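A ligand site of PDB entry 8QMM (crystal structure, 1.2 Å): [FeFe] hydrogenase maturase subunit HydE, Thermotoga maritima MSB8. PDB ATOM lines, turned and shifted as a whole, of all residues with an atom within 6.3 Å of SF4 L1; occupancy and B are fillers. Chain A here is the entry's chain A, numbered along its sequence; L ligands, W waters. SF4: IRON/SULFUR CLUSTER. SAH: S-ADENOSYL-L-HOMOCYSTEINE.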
ATOM      1  N   VAL A  72      -8.940  -3.354 -14.716  1.00  0.00           N
ATOM      2  CA  VAL A  72      -8.996  -3.779 -13.320  1.00  0.00           C
ATOM      3  C   VAL A  72      -9.182  -2.553 -12.476  1.00  0.00           C
ATOM      4  O   VAL A  72      -8.451  -1.564 -12.595  1.00  0.00           O
ATOM      5  CB  VAL A  72      -7.717  -4.511 -12.943  1.00  0.00           C
ATOM      6  CG1 VAL A  72      -7.668  -4.851 -11.477  1.00  0.00           C
ATOM      7  CG2 VAL A  72      -7.523  -5.781 -13.791  1.00  0.00           C
ATOM      8  N   CYS A  73     -10.127  -2.598 -11.508  1.00  0.00           N
ATOM      9  CA  CYS A  73     -10.304  -1.469 -10.605  1.00  0.00           C
ATOM     10  C   CYS A  73     -10.607  -1.942  -9.203  1.00  0.00           C
ATOM     11  O   CYS A  73     -11.436  -2.819  -8.987  1.00  0.00           O
ATOM     12  CB  CYS A  73     -11.391  -0.526 -11.091  1.00  0.00           C
ATOM     13  SG  CYS A  73     -11.346   1.041 -10.166  1.00  0.00           S
ATOM     14  N   ARG A  74      -9.933  -1.307  -8.234  1.00  0.00           N
ATOM     15  CA  ARG A  74     -10.173  -1.573  -6.826  1.00  0.00           C
ATOM     16  C   ARG A  74     -11.409  -0.851  -6.310  1.00  0.00           C
ATOM     17  O   ARG A  74     -11.884  -1.186  -5.190  1.00  0.00           O
ATOM     18  CB  ARG A  74      -8.944  -1.192  -6.009  1.00  0.00           C
ATOM     19  CG  ARG A  74      -8.657   0.284  -5.996  1.00  0.00           C
ATOM     20  CD  ARG A  74      -7.411   0.642  -5.266  1.00  0.00           C
ATOM     21  NE  ARG A  74      -7.143   2.053  -5.365  1.00  0.00           N
ATOM     22  CZ  ARG A  74      -6.234   2.691  -4.648  1.00  0.00           C
ATOM     23  NH1 ARG A  74      -5.454   2.044  -3.765  1.00  0.00           N
ATOM     24  NH2 ARG A  74      -6.091   3.988  -4.803  1.00  0.00           N
ATOM     25  N   LYS A  75     -11.941   0.137  -7.007  1.00  0.00           N
ATOM     26  CA  LYS A  75     -13.085   0.923  -6.547  1.00  0.00           C
ATOM     27  C   LYS A  75     -14.362   0.329  -7.084  1.00  0.00           C
ATOM     28  O   LYS A  75     -14.378  -0.638  -7.844  1.00  0.00           O
ATOM     29  CB  LYS A  75     -12.910   2.392  -6.912  1.00  0.00           C
ATOM     30  CG  LYS A  75     -11.943   3.099  -5.952  1.00  0.00           C
ATOM     31  CD  LYS A  75     -11.873   4.584  -6.230  1.00  0.00           C
ATOM     32  CE  LYS A  75     -11.231   5.423  -5.163  1.00  0.00           C
ATOM     33  NZ  LYS A  75      -9.917   4.914  -4.764  1.00  0.00           N
ATOM     34  N   ASN A  76     -15.482   0.915  -6.629  1.00  0.00           N
ATOM     35  CA  ASN A  76     -16.801   0.356  -6.831  1.00  0.00           C
ATOM     36  C   ASN A  76     -17.811   1.438  -7.213  1.00  0.00           C
ATOM     37  O   ASN A  76     -18.989   1.356  -6.811  1.00  0.00           O
ATOM     38  CB  ASN A  76     -17.264  -0.412  -5.597  1.00  0.00           C
ATOM     39  CG  ASN A  76     -18.162  -1.580  -5.901  1.00  0.00           C
ATOM     40  OD1 ASN A  76     -18.171  -2.158  -7.005  1.00  0.00           O
ATOM     41  ND2 ASN A  76     -18.946  -1.932  -4.927  1.00  0.00           N
ATOM     42  N   CYS A  77     -17.419   2.447  -7.988  1.00  0.00           N
ATOM     43  CA  CYS A  77     -18.296   3.546  -8.341  1.00  0.00           C
ATOM     44  C   CYS A  77     -19.601   3.020  -8.923  1.00  0.00           C
ATOM     45  O   CYS A  77     -19.590   2.130  -9.768  1.00  0.00           O
ATOM     46  CB  CYS A  77     -17.610   4.478  -9.324  1.00  0.00           C
ATOM     47  SG  CYS A  77     -15.975   5.092  -8.737  1.00  0.00           S
ATOM     48  N   TYR A  79     -21.767   4.083 -10.954  1.00  0.00           N
ATOM     49  CA  TYR A  79     -22.083   4.345 -12.363  1.00  0.00           C
ATOM     50  C   TYR A  79     -21.250   3.536 -13.348  1.00  0.00           C
ATOM     51  O   TYR A  79     -21.601   3.468 -14.525  1.00  0.00           O
ATOM     52  CB  TYR A  79     -21.940   5.851 -12.655  1.00  0.00           C
ATOM     53  CG  TYR A  79     -20.675   6.449 -12.110  1.00  0.00           C
ATOM     54  CD1 TYR A  79     -19.480   6.304 -12.765  1.00  0.00           C
ATOM     55  CD2 TYR A  79     -20.699   7.154 -10.942  1.00  0.00           C
ATOM     56  CE1 TYR A  79     -18.304   6.855 -12.252  1.00  0.00           C
ATOM     57  CE2 TYR A  79     -19.553   7.719 -10.426  1.00  0.00           C
ATOM     58  CZ  TYR A  79     -18.357   7.549 -11.079  1.00  0.00           C
ATOM     59  OH  TYR A  79     -17.236   8.144 -10.527  1.00  0.00           O
ATOM     60  N   CYS A  80     -20.125   2.987 -12.909  1.00  0.00           N
ATOM     61  CA  CYS A  80     -19.084   2.554 -13.835  1.00  0.00           C
ATOM     62  C   CYS A  80     -19.081   1.049 -14.062  1.00  0.00           C
ATOM     63  O   CYS A  80     -19.083   0.251 -13.110  1.00  0.00           O
ATOM     64  CB  CYS A  80     -17.719   2.973 -13.258  1.00  0.00           C
ATOM     65  SG  CYS A  80     -16.328   2.559 -14.332  1.00  0.00           S
ATOM     66  N   GLY A  81     -19.057   0.656 -15.333  1.00  0.00           N
ATOM     67  CA  GLY A  81     -19.032  -0.750 -15.674  1.00  0.00           C
ATOM     68  C   GLY A  81     -17.772  -1.475 -15.158  1.00  0.00           C
ATOM     69  O   GLY A  81     -17.782  -2.701 -15.060  1.00  0.00           O
ATOM     70  N   LEU A  82     -16.688  -0.750 -14.822  1.00  0.00           N
ATOM     71  CA  LEU A  82     -15.477  -1.411 -14.327  1.00  0.00           C
ATOM     72  C   LEU A  82     -15.489  -1.582 -12.841  1.00  0.00           C
ATOM     73  O   LEU A  82     -14.527  -2.137 -12.283  1.00  0.00           O
ATOM     74  CB  LEU A  82     -14.238  -0.608 -14.712  1.00  0.00           C
ATOM     75  CG  LEU A  82     -14.083  -0.345 -16.215  1.00  0.00           C
ATOM     76  CD1 LEU A  82     -12.696   0.215 -16.512  1.00  0.00           C
ATOM     77  CD2 LEU A  82     -14.433  -1.478 -17.117  1.00  0.00           C
ATOM     78  N   ARG A  83     -16.543  -1.167 -12.149  1.00  0.00           N
ATOM     79  CA  ARG A  83     -16.596  -1.332 -10.708  1.00  0.00           C
ATOM     80  C   ARG A  83     -16.268  -2.765 -10.330  1.00  0.00           C
ATOM     81  O   ARG A  83     -16.649  -3.722 -10.986  1.00  0.00           O
ATOM     82  CB  ARG A  83     -17.974  -0.894 -10.199  1.00  0.00           C
ATOM     83  CG  ARG A  83     -19.120  -1.797 -10.672  1.00  0.00           C
ATOM     84  CD  ARG A  83     -20.471  -1.058 -10.464  1.00  0.00           C
ATOM     85  NE  ARG A  83     -20.630  -0.519  -9.137  1.00  0.00           N
ATOM     86  CZ  ARG A  83     -21.151  -1.123  -8.090  1.00  0.00           C
ATOM     87  NH1 ARG A  83     -21.644  -2.327  -8.186  1.00  0.00           N
ATOM     88  NH2 ARG A  83     -21.164  -0.500  -6.916  1.00  0.00           N
ATOM     89  N   ARG A  84     -15.600  -2.928  -9.178  1.00  0.00           N
ATOM     90  CA  ARG A  84     -15.096  -4.255  -8.831  1.00  0.00           C
ATOM     91  C   ARG A  84     -16.224  -5.259  -8.672  1.00  0.00           C
ATOM     92  O   ARG A  84     -15.992  -6.461  -8.885  1.00  0.00           O
ATOM     93  CB  ARG A  84     -14.256  -4.137  -7.547  1.00  0.00           C
ATOM     94  CG  ARG A  84     -15.017  -3.753  -6.313  1.00  0.00           C
ATOM     95  CD  ARG A  84     -14.165  -3.780  -5.088  1.00  0.00           C
ATOM     96  NE  ARG A  84     -14.938  -3.481  -3.888  1.00  0.00           N
ATOM     97  CZ  ARG A  84     -15.080  -2.252  -3.360  1.00  0.00           C
ATOM     98  NH1 ARG A  84     -14.321  -1.248  -3.736  1.00  0.00           N
ATOM     99  NH2 ARG A  84     -16.021  -2.060  -2.453  1.00  0.00           N
ATOM    100  N   SER A 118      -6.652   3.867 -16.984  1.00  0.00           N
ATOM    101  CA  SER A 118      -6.967   2.552 -16.477  1.00  0.00           C
ATOM    102  C   SER A 118      -7.986   2.663 -15.357  1.00  0.00           C
ATOM    103  O   SER A 118      -8.194   3.734 -14.788  1.00  0.00           O
ATOM    104  CB  SER A 118      -5.727   1.864 -15.991  1.00  0.00           C
ATOM    105  OG  SER A 118      -5.090   2.542 -14.914  1.00  0.00           O
ATOM    106  N   GLY A 119      -8.538   1.505 -14.989  1.00  0.00           N
ATOM    107  CA  GLY A 119      -9.071   1.376 -13.637  1.00  0.00           C
ATOM    108  C   GLY A 119      -7.988   1.607 -12.624  1.00  0.00           C
ATOM    109  O   GLY A 119      -6.789   1.639 -12.953  1.00  0.00           O
ATOM    110  N   GLU A 120      -8.380   1.776 -11.367  1.00  0.00           N
ATOM    111  CA  GLU A 120      -7.382   1.886 -10.308  1.00  0.00           C
ATOM    112  C   GLU A 120      -6.844   0.485 -10.037  1.00  0.00           C
ATOM    113  O   GLU A 120      -7.344  -0.241  -9.168  1.00  0.00           O
ATOM    114  CB  GLU A 120      -7.964   2.519  -9.026  1.00  0.00           C
ATOM    115  CG  GLU A 120      -8.344   3.970  -9.204  1.00  0.00           C
ATOM    116  CD  GLU A 120      -8.606   4.671  -7.906  1.00  0.00           C
ATOM    117  OE1 GLU A 120      -8.398   4.056  -6.847  1.00  0.00           O
ATOM    118  OE2 GLU A 120      -9.021   5.858  -7.965  1.00  0.00           O
ATOM    119  N   GLY A 148      -6.750   7.630 -11.727  1.00  0.00           N
ATOM    120  CA  GLY A 148      -7.513   7.715 -10.484  1.00  0.00           C
ATOM    121  C   GLY A 148      -6.752   8.339  -9.341  1.00  0.00           C
ATOM    122  O   GLY A 148      -5.816   9.123  -9.542  1.00  0.00           O
ATOM    123  N   GLU A 171     -16.326  14.513 -11.154  1.00  0.00           N
ATOM    124  CA  GLU A 171     -17.520  13.693 -11.262  1.00  0.00           C
ATOM    125  C   GLU A 171     -18.779  14.438 -10.882  1.00  0.00           C
ATOM    126  O   GLU A 171     -19.708  14.534 -11.678  1.00  0.00           O
ATOM    127  CB  GLU A 171     -17.402  12.377 -10.505  1.00  0.00           C
ATOM    128  CG  GLU A 171     -16.103  11.598 -10.759  1.00  0.00           C
ATOM    129  CD  GLU A 171     -15.832  11.178 -12.180  1.00  0.00           C
ATOM    130  OE1 GLU A 171     -16.576  11.507 -13.115  1.00  0.00           O
ATOM    131  OE2 GLU A 171     -14.814  10.490 -12.357  1.00  0.00           O
ATOM    132  N   ARG A 182     -19.727   7.101  -5.118  1.00  0.00           N
ATOM    133  CA  ARG A 182     -18.321   6.700  -5.096  1.00  0.00           C
ATOM    134  C   ARG A 182     -18.010   6.291  -3.670  1.00  0.00           C
ATOM    135  O   ARG A 182     -17.347   7.011  -2.925  1.00  0.00           O
ATOM    136  CB  ARG A 182     -17.438   7.822  -5.611  1.00  0.00           C
ATOM    137  CG  ARG A 182     -17.928   8.368  -6.958  1.00  0.00           C
ATOM    138  CD  ARG A 182     -16.897   9.290  -7.619  1.00  0.00           C
ATOM    139  NE  ARG A 182     -15.708   8.566  -8.027  1.00  0.00           N
ATOM    140  CZ  ARG A 182     -14.508   8.684  -7.466  1.00  0.00           C
ATOM    141  NH1 ARG A 182     -14.195   9.672  -6.638  1.00  0.00           N
ATOM    142  NH2 ARG A 182     -13.544   7.800  -7.809  1.00  0.00           N
ATOM    143  N   ARG A 190     -11.017  13.620  -3.737  1.00  0.00           N
ATOM    144  CA  ARG A 190     -10.896  13.892  -5.156  1.00  0.00           C
ATOM    145  C   ARG A 190     -10.249  15.266  -5.352  1.00  0.00           C
ATOM    146  O   ARG A 190      -9.341  15.445  -6.169  1.00  0.00           O
ATOM    147  CB  ARG A 190     -12.300  13.804  -5.847  1.00  0.00           C
ATOM    148  CG  ARG A 190     -12.251  13.644  -7.340  1.00  0.00           C
ATOM    149  CD  ARG A 190     -11.896  12.274  -7.699  1.00  0.00           C
ATOM    150  NE  ARG A 190     -12.160  11.973  -9.116  1.00  0.00           N
ATOM    151  CZ  ARG A 190     -11.816  10.832  -9.706  1.00  0.00           C
ATOM    152  NH1 ARG A 190     -11.290   9.877  -8.997  1.00  0.00           N
ATOM    153  NH2 ARG A 190     -11.974  10.705 -11.013  1.00  0.00           N
ATOM    154  N   TYR A 313     -13.169  -2.545 -22.188  1.00  0.00           N
ATOM    155  CA  TYR A 313     -13.067  -1.329 -21.379  1.00  0.00           C
ATOM    156  C   TYR A 313     -14.429  -0.647 -21.372  1.00  0.00           C
ATOM    157  O   TYR A 313     -14.634   0.437 -21.891  1.00  0.00           O
ATOM    158  CB  TYR A 313     -11.944  -0.424 -21.865  1.00  0.00           C
ATOM    159  CG  TYR A 313     -11.550   0.600 -20.844  1.00  0.00           C
ATOM    160  CD1 TYR A 313     -10.702   0.315 -19.786  1.00  0.00           C
ATOM    161  CD2 TYR A 313     -12.000   1.902 -20.967  1.00  0.00           C
ATOM    162  CE1 TYR A 313     -10.281   1.261 -18.883  1.00  0.00           C
ATOM    163  CE2 TYR A 313     -11.591   2.890 -20.088  1.00  0.00           C
ATOM    164  CZ  TYR A 313     -10.749   2.561 -19.053  1.00  0.00           C
ATOM    165  OH  TYR A 313     -10.343   3.535 -18.194  1.00  0.00           O
ATOM    166  N   LEU A 315     -16.874   1.091 -19.792  1.00  0.00           N
ATOM    167  CA  LEU A 315     -17.315   2.053 -18.775  1.00  0.00           C
ATOM    168  C   LEU A 315     -18.825   2.176 -18.867  1.00  0.00           C
ATOM    169  O   LEU A 315     -19.514   2.262 -17.816  1.00  0.00           O
ATOM    170  CB  LEU A 315     -16.729   3.443 -19.021  1.00  0.00           C
ATOM    171  CG  LEU A 315     -15.221   3.566 -19.025  1.00  0.00           C
ATOM    172  CD1 LEU A 315     -14.859   4.983 -19.448  1.00  0.00           C
ATOM    173  CD2 LEU A 315     -14.611   3.261 -17.663  1.00  0.00           C
HETATM  174 FE1  SF4 L   1     -14.704   3.185 -12.882  1.00  0.00          FE
HETATM  175 FE2  SF4 L   1     -12.793   2.476 -11.129  1.00  0.00          FE
HETATM  176 FE3  SF4 L   1     -14.591   4.376 -10.462  1.00  0.00          FE
HETATM  177 FE4  SF4 L   1     -12.567   5.015 -12.395  1.00  0.00          FE
HETATM  178  S1  SF4 L   1     -12.367   4.495 -10.093  1.00  0.00           S
HETATM  179  S2  SF4 L   1     -14.865   5.449 -12.493  1.00  0.00           S
HETATM  180  S3  SF4 L   1     -12.537   2.837 -13.362  1.00  0.00           S
HETATM  181  S4  SF4 L   1     -15.026   2.153 -10.829  1.00  0.00           S
HETATM  182  N   SAH L   2     -10.415   5.210 -12.892  1.00  0.00           N
HETATM  183  CA  SAH L   2     -10.057   6.547 -13.378  1.00  0.00           C
HETATM  184  CB  SAH L   2     -10.006   6.557 -14.904  1.00  0.00           C
HETATM  185  CG  SAH L   2     -11.014   5.697 -15.662  1.00  0.00           C
HETATM  186  SD  SAH L   2     -12.762   6.084 -15.444  1.00  0.00           S
HETATM  187  C   SAH L   2     -11.020   7.569 -12.791  1.00  0.00           C
HETATM  188  O   SAH L   2     -10.716   8.776 -12.853  1.00  0.00           O
HETATM  189  OXT SAH L   2     -12.074   7.108 -12.274  1.00  0.00           O
HETATM  190  C5' SAH L   2     -12.839   7.531 -16.558  1.00  0.00           C
HETATM  191  C4' SAH L   2     -14.133   8.358 -16.512  1.00  0.00           C
HETATM  192  O4' SAH L   2     -15.175   7.621 -17.148  1.00  0.00           O
HETATM  193  C3' SAH L   2     -14.732   8.705 -15.198  1.00  0.00           C
HETATM  194  O3' SAH L   2     -14.103   9.868 -14.709  1.00  0.00           O
HETATM  195  C2' SAH L   2     -16.209   8.963 -15.504  1.00  0.00           C
HETATM  196  O2' SAH L   2     -16.522  10.338 -15.619  1.00  0.00           O
HETATM  197  C1' SAH L   2     -16.393   8.247 -16.848  1.00  0.00           C
HETATM  198  N9  SAH L   2     -17.482   7.289 -16.757  1.00  0.00           N
HETATM  199  C8  SAH L   2     -17.518   6.169 -15.968  1.00  0.00           C
HETATM  200  N7  SAH L   2     -18.689   5.574 -16.023  1.00  0.00           N
HETATM  201  C5  SAH L   2     -19.489   6.345 -16.837  1.00  0.00           C
HETATM  202  C6  SAH L   2     -20.804   6.234 -17.273  1.00  0.00           C
HETATM  203  N6  SAH L   2     -21.594   5.230 -16.863  1.00  0.00           N
HETATM  204  N1  SAH L   2     -21.296   7.207 -18.089  1.00  0.00           N
HETATM  205  C2  SAH L   2     -20.474   8.185 -18.494  1.00  0.00           C
HETATM  206  N3  SAH L   2     -19.201   8.341 -18.157  1.00  0.00           N
HETATM  207  C4  SAH L   2     -18.722   7.409 -17.292  1.00  0.00           C
HETATM  208  O   HOH W   1     -14.565   8.231 -10.862  1.00  0.00           O
HETATM  209  O   HOH W   2     -10.692   7.213  -9.569  1.00  0.00           O
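Water W2 lies within hydrogen-bond range of the side-chain carboxylate (OE2) of Glu 120 (2.7 Å), the guanidinium group (NH1) of Arg 190 (2.8 Å), a sulfur (S1) of SF4 L1 (3.2 Å) and the guanidinium group (NH2) of Arg 182 (3.4 Å).
Water W1 lies within hydrogen-bond range of OH of Tyr 79, OE2 of Glu 171, NE of Arg 182 and S2 of SF4 L1.
Lys 75 touches SF4 L1 (CB to S1, 3.9 Å).
CE1 of Tyr 79 touches S2 of SF4 L1 (3.7 Å).
Arg 83 touches SF4 L1 (CA to S4, 3.8 Å).
CA of Gly 119 touches S3 of SF4 L1, at 3.8 Å.
Seven residues have an atom within 4 Å of SF4 L1: Cys 73, Lys 75, Cys 77, Tyr 79, Cys 80, Arg 83 and Gly 119.
Along chain A the residues within 4 Å of SF4 L1 span positions 73 to 119.
OXT of SAH L2 binds FE4 of SF4 L1, at 2.2 Å.
An iron atom (FE3) of SF4 L1 is bound by the side-chain sulfur (SG) of Cys 77 (2.3 Å).
FE2 of SF4 L1 is bound by SG of Cys 73 (2.3 Å).
O of SAH L2 lies within salt-bridge range of NH2 of Arg 190 (2.9 Å).
The side-chain sulfur (SG) of Cys 80 is bound to an iron atom (FE1) of SF4 L1 (2.3 Å).
The backbone carbonyl oxygen of Tyr 79 sits at hydrogen-bond distance from a nitrogen (N6) of SAH L2, 2.9 Å away.
S4 of SF4 L1 lies close to N of Cys 77 (3.7 Å).
The backbone carbonyl oxygen (O) of Ser 118 sits close to a nitrogen (N) of SAH L2, at 3.3 Å.
The side-chain carboxylate (OE2) of Glu 171 lies within hydrogen-bond range of an oxygen (O3') of SAH L2 (2.5 Å).
SG of Cys 80 lies close to N of Leu 82 (3.4 Å).
The guanidinium group (NE) of Arg 83 lies within hydrogen-bond range of the backbone carbonyl oxygen (O) of Cys 77 (2.9 Å).
The side-chain sulfur (SG) of Cys 73 sits close to the backbone NH (N) of Lys 75 (3.3 Å).
OH of Tyr 79 sits at hydrogen-bond distance from NE of Arg 182 (3.0 Å).
The side-chain sulfur (SG) of Cys 77 lies close to the guanidinium group (NE) of Arg 182 (3.6 Å).
The guanidinium group (NH2) of Arg 83 is in hydrogen-bond range of the backbone carbonyl oxygen (O) of Asn 76 (2.9 Å).
SG of Cys 73 sits close to N of Glu 120, at 3.3 Å.
O of Lys 75 is in hydrogen-bond range of N of Arg 84.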
